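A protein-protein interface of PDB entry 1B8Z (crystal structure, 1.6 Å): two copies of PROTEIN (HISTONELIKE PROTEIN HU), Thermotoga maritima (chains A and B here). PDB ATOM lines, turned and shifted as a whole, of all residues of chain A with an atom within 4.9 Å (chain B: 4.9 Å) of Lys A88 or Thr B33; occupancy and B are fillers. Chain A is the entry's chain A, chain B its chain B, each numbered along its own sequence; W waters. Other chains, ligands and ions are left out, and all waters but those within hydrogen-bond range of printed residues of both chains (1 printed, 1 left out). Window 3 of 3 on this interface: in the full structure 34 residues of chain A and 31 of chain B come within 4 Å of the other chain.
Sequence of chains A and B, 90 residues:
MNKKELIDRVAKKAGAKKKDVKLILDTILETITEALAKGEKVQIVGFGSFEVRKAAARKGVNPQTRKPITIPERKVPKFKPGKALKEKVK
Phe A47 touches Leu B29 (CG to CD2, 3.8 Å). Leu A85 touches Thr B33. CD of Lys A88 touches CG2 of Thr B33, 3.4 Å away. Lys A88 touches Ala B37. Val A89 touches Leu B36. Ala B37 touches Val A89 (N to CG1, 3.9 Å).
No position is printed for both chains. Of the 6 pairs that touch across the chains among the printed residues, none has its exchanged pair printed and touching as well.
Of the printed residues of chain B, Phe A47 touches Leu B29. Of chain B, only Thr B33 (3.4 Å) and Ala B37 (3.8 Å) come within 4 Å of Lys A88. Printed residues of chain A within 4 Å of Leu B29: Phe A47. Glu B30 touches none of the printed residues of chain A. Of the printed residues of chain A, Thr B33 touches Leu A85 (3.7 Å) and Lys A88 (3.4 Å). Printed residues of chain A within 4 Å of Leu B36: Val A89. Of the printed residues of chain A, Ala B37 touches Lys A88 (3.8 Å) and Val A89 (3.9 Å). The nearest residue of chain A that does not touch Thr B33 is Phe A47 (4.1 Å). The nearest printed residue of chain A that does not touch Ala B37 is Lys A90 (6.2 Å).
Of the 9 printed residues of chain A, 4 touch a printed residue of chain B. Printed residues of chain A that touch a printed residue of chain B: Phe A47, Leu A85, Lys A88 and Val A89. Hydrophobic or aromatic side chains of chain B that line the printed part of chain A: Leu B29, Leu B36 and Ala B37. Among the printed residues, no Asp or Glu carboxylate lies within 4 Å of a Lys or Arg side-chain nitrogen of the other chain.
Water W1 lies within hydrogen-bond range of the side-chain amino group (NZ) of Lys A88 (2.6 Å), the backbone carbonyl oxygen (O) of Gly A46 (2.8 Å) and the side-chain hydroxyl (OG1) of Thr B33 (3.4 Å).
OG1 of Thr B33 lies within hydrogen-bond range of O of Leu B29 (2.9 Å).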
ATOM      1  N   GLY A  46      -1.211  20.379 -18.322  1.00  0.00           N
ATOM      2  CA  GLY A  46      -2.546  20.280 -18.919  1.00  0.00           C
ATOM      3  C   GLY A  46      -3.522  19.467 -18.088  1.00  0.00           C
ATOM      4  O   GLY A  46      -4.641  19.198 -18.552  1.00  0.00           O
ATOM      5  N   PHE A  47      -3.133  19.080 -16.878  1.00  0.00           N
ATOM      6  CA  PHE A  47      -4.020  18.331 -15.996  1.00  0.00           C
ATOM      7  C   PHE A  47      -3.932  18.879 -14.592  1.00  0.00           C
ATOM      8  O   PHE A  47      -4.898  19.441 -14.049  1.00  0.00           O
ATOM      9  CB  PHE A  47      -3.768  16.820 -16.075  1.00  0.00           C
ATOM     10  CG  PHE A  47      -4.806  16.028 -15.328  1.00  0.00           C
ATOM     11  CD1 PHE A  47      -6.080  15.852 -15.847  1.00  0.00           C
ATOM     12  CD2 PHE A  47      -4.491  15.461 -14.111  1.00  0.00           C
ATOM     13  CE1 PHE A  47      -7.014  15.118 -15.141  1.00  0.00           C
ATOM     14  CE2 PHE A  47      -5.430  14.729 -13.397  1.00  0.00           C
ATOM     15  CZ  PHE A  47      -6.695  14.559 -13.922  1.00  0.00           C
ATOM     16  N   ALA A  84      -5.874  24.528 -17.653  1.00  0.00           N
ATOM     17  CA  ALA A  84      -6.599  23.835 -18.731  1.00  0.00           C
ATOM     18  C   ALA A  84      -7.746  22.983 -18.194  1.00  0.00           C
ATOM     19  O   ALA A  84      -8.857  23.014 -18.740  1.00  0.00           O
ATOM     20  CB  ALA A  84      -5.642  22.922 -19.500  1.00  0.00           C
ATOM     21  N   LEU A  85      -7.501  22.222 -17.124  1.00  0.00           N
ATOM     22  CA  LEU A  85      -8.564  21.402 -16.542  1.00  0.00           C
ATOM     23  C   LEU A  85      -9.675  22.278 -15.970  1.00  0.00           C
ATOM     24  O   LEU A  85     -10.857  22.056 -16.257  1.00  0.00           O
ATOM     25  CB  LEU A  85      -8.011  20.457 -15.477  1.00  0.00           C
ATOM     26  CG  LEU A  85      -9.012  19.600 -14.711  1.00  0.00           C
ATOM     27  CD1 LEU A  85      -9.805  18.699 -15.652  1.00  0.00           C
ATOM     28  CD2 LEU A  85      -8.308  18.772 -13.645  1.00  0.00           C
ATOM     29  N   LYS A  86      -9.314  23.310 -15.224  1.00  0.00           N
ATOM     30  CA  LYS A  86     -10.287  24.250 -14.666  1.00  0.00           C
ATOM     31  C   LYS A  86     -11.145  24.902 -15.743  1.00  0.00           C
ATOM     32  O   LYS A  86     -12.369  25.004 -15.597  1.00  0.00           O
ATOM     33  CB  LYS A  86      -9.560  25.342 -13.886  1.00  0.00           C
ATOM     34  CG  LYS A  86      -9.033  24.970 -12.518  1.00  0.00           C
ATOM     35  CD  LYS A  86      -7.844  25.854 -12.162  1.00  0.00           C
ATOM     36  CE  LYS A  86      -7.870  26.252 -10.696  1.00  0.00           C
ATOM     37  NZ  LYS A  86      -6.838  27.292 -10.409  1.00  0.00           N
ATOM     38  N   GLU A  87     -10.543  25.309 -16.862  1.00  0.00           N
ATOM     39  CA  GLU A  87     -11.300  25.917 -17.953  1.00  0.00           C
ATOM     40  C   GLU A  87     -12.266  24.926 -18.587  1.00  0.00           C
ATOM     41  O   GLU A  87     -13.405  25.273 -18.926  1.00  0.00           O
ATOM     42  CB  GLU A  87     -10.365  26.486 -19.023  1.00  0.00           C
ATOM     43  N   LYS A  88     -11.849  23.670 -18.738  1.00  0.00           N
ATOM     44  CA  LYS A  88     -12.686  22.647 -19.345  1.00  0.00           C
ATOM     45  C   LYS A  88     -13.890  22.237 -18.514  1.00  0.00           C
ATOM     46  O   LYS A  88     -14.895  21.811 -19.099  1.00  0.00           O
ATOM     47  CB  LYS A  88     -11.853  21.395 -19.662  1.00  0.00           C
ATOM     48  CG  LYS A  88     -11.088  21.506 -20.970  1.00  0.00           C
ATOM     49  CD  LYS A  88     -10.227  20.285 -21.231  1.00  0.00           C
ATOM     50  CE  LYS A  88      -8.818  20.663 -21.656  1.00  0.00           C
ATOM     51  NZ  LYS A  88      -7.949  19.463 -21.829  1.00  0.00           N
ATOM     52  N   VAL A  89     -13.825  22.330 -17.192  1.00  0.00           N
ATOM     53  CA  VAL A  89     -14.922  21.890 -16.342  1.00  0.00           C
ATOM     54  C   VAL A  89     -15.754  23.026 -15.775  1.00  0.00           C
ATOM     55  O   VAL A  89     -16.781  22.782 -15.130  1.00  0.00           O
ATOM     56  CB  VAL A  89     -14.435  21.009 -15.167  1.00  0.00           C
ATOM     57  CG1 VAL A  89     -13.615  19.835 -15.675  1.00  0.00           C
ATOM     58  CG2 VAL A  89     -13.648  21.830 -14.161  1.00  0.00           C
ATOM     59  N   LYS A  90     -15.329  24.265 -15.995  1.00  0.00           N
ATOM     60  CA  LYS A  90     -16.088  25.416 -15.503  1.00  0.00           C
ATOM     61  C   LYS A  90     -17.485  25.395 -16.124  1.00  0.00           C
ATOM     62  O   LYS A  90     -18.438  25.689 -15.371  1.00  0.00           O
ATOM     63  OXT LYS A  90     -17.607  25.092 -17.332  1.00  0.00           O
ATOM     64  N   LEU B  29      -6.366  10.691 -19.058  1.00  0.00           N
ATOM     65  CA  LEU B  29      -6.572  12.080 -18.663  1.00  0.00           C
ATOM     66  C   LEU B  29      -7.732  12.710 -19.439  1.00  0.00           C
ATOM     67  O   LEU B  29      -8.477  13.430 -18.772  1.00  0.00           O
ATOM     68  CB  LEU B  29      -5.317  12.931 -18.858  1.00  0.00           C
ATOM     69  CG  LEU B  29      -4.106  12.396 -18.084  1.00  0.00           C
ATOM     70  CD1 LEU B  29      -2.879  13.198 -18.511  1.00  0.00           C
ATOM     71  CD2 LEU B  29      -4.332  12.430 -16.582  1.00  0.00           C
ATOM     72  N   GLU B  30      -7.867  12.396 -20.710  1.00  0.00           N
ATOM     73  CA  GLU B  30      -8.986  12.936 -21.497  1.00  0.00           C
ATOM     74  C   GLU B  30     -10.296  12.350 -20.986  1.00  0.00           C
ATOM     75  O   GLU B  30     -11.272  13.121 -20.858  1.00  0.00           O
ATOM     76  CB  GLU B  30      -8.761  12.537 -22.953  1.00  0.00           C
ATOM     77  CG  GLU B  30      -7.625  13.372 -23.541  1.00  0.00           C
ATOM     78  CD  GLU B  30      -7.173  12.965 -24.925  1.00  0.00           C
ATOM     79  OE1 GLU B  30      -7.853  12.166 -25.601  1.00  0.00           O
ATOM     80  OE2 GLU B  30      -6.104  13.463 -25.355  1.00  0.00           O
ATOM     81  N   THR B  31     -10.296  11.069 -20.641  1.00  0.00           N
ATOM     82  CA  THR B  31     -11.548  10.460 -20.137  1.00  0.00           C
ATOM     83  C   THR B  31     -11.969  11.047 -18.818  1.00  0.00           C
ATOM     84  O   THR B  31     -13.155  11.300 -18.573  1.00  0.00           O
ATOM     85  CB  THR B  31     -11.410   8.942 -20.069  1.00  0.00           C
ATOM     86  OG1 THR B  31     -11.106   8.495 -21.399  1.00  0.00           O
ATOM     87  CG2 THR B  31     -12.682   8.246 -19.599  1.00  0.00           C
ATOM     88  N   ILE B  32     -11.040  11.270 -17.877  1.00  0.00           N
ATOM     89  CA  ILE B  32     -11.376  11.894 -16.612  1.00  0.00           C
ATOM     90  C   ILE B  32     -11.851  13.323 -16.838  1.00  0.00           C
ATOM     91  O   ILE B  32     -12.861  13.754 -16.260  1.00  0.00           O
ATOM     92  CB  ILE B  32     -10.148  11.871 -15.663  1.00  0.00           C
ATOM     93  CG1 ILE B  32      -9.857  10.428 -15.299  1.00  0.00           C
ATOM     94  CG2 ILE B  32     -10.403  12.788 -14.462  1.00  0.00           C
ATOM     95  CD1 ILE B  32      -8.532  10.291 -14.509  1.00  0.00           C
ATOM     96  N   THR B  33     -11.183  14.093 -17.683  1.00  0.00           N
ATOM     97  CA  THR B  33     -11.584  15.484 -17.959  1.00  0.00           C
ATOM     98  C   THR B  33     -12.995  15.526 -18.534  1.00  0.00           C
ATOM     99  O   THR B  33     -13.768  16.366 -18.063  1.00  0.00           O
ATOM    100  CB  THR B  33     -10.591  16.087 -18.963  1.00  0.00           C
ATOM    101  OG1 THR B  33      -9.307  16.128 -18.326  1.00  0.00           O
ATOM    102  CG2 THR B  33     -10.998  17.495 -19.374  1.00  0.00           C
ATOM    103  N   GLU B  34     -13.291  14.651 -19.482  1.00  0.00           N
ATOM    104  CA  GLU B  34     -14.631  14.636 -20.096  1.00  0.00           C
ATOM    105  C   GLU B  34     -15.686  14.302 -19.050  1.00  0.00           C
ATOM    106  O   GLU B  34     -16.745  14.949 -19.014  1.00  0.00           O
ATOM    107  CB  GLU B  34     -14.715  13.623 -21.228  1.00  0.00           C
ATOM    108  CG  GLU B  34     -13.925  13.977 -22.472  1.00  0.00           C
ATOM    109  CD  GLU B  34     -13.757  12.827 -23.445  1.00  0.00           C
ATOM    110  OE1 GLU B  34     -14.479  11.810 -23.360  1.00  0.00           O
ATOM    111  OE2 GLU B  34     -12.875  12.932 -24.328  1.00  0.00           O
ATOM    112  N   ALA B  35     -15.422  13.348 -18.160  1.00  0.00           N
ATOM    113  CA  ALA B  35     -16.394  12.998 -17.118  1.00  0.00           C
ATOM    114  C   ALA B  35     -16.662  14.174 -16.191  1.00  0.00           C
ATOM    115  O   ALA B  35     -17.821  14.497 -15.862  1.00  0.00           O
ATOM    116  CB  ALA B  35     -15.887  11.796 -16.319  1.00  0.00           C
ATOM    117  N   LEU B  36     -15.609  14.875 -15.775  1.00  0.00           N
ATOM    118  CA  LEU B  36     -15.733  16.034 -14.897  1.00  0.00           C
ATOM    119  C   LEU B  36     -16.485  17.169 -15.595  1.00  0.00           C
ATOM    120  O   LEU B  36     -17.261  17.878 -14.937  1.00  0.00           O
ATOM    121  CB  LEU B  36     -14.368  16.551 -14.431  1.00  0.00           C
ATOM    122  CG  LEU B  36     -13.643  15.553 -13.512  1.00  0.00           C
ATOM    123  CD1 LEU B  36     -12.250  16.090 -13.206  1.00  0.00           C
ATOM    124  CD2 LEU B  36     -14.428  15.245 -12.266  1.00  0.00           C
ATOM    125  N   ALA B  37     -16.276  17.303 -16.894  1.00  0.00           N
ATOM    126  CA  ALA B  37     -16.947  18.358 -17.674  1.00  0.00           C
ATOM    127  C   ALA B  37     -18.455  18.141 -17.689  1.00  0.00           C
ATOM    128  O   ALA B  37     -19.200  19.142 -17.731  1.00  0.00           O
ATOM    129  CB  ALA B  37     -16.414  18.380 -19.093  1.00  0.00           C
HETATM  130  O   HOH W   1      -7.148  18.456 -19.540  1.00  0.00           O
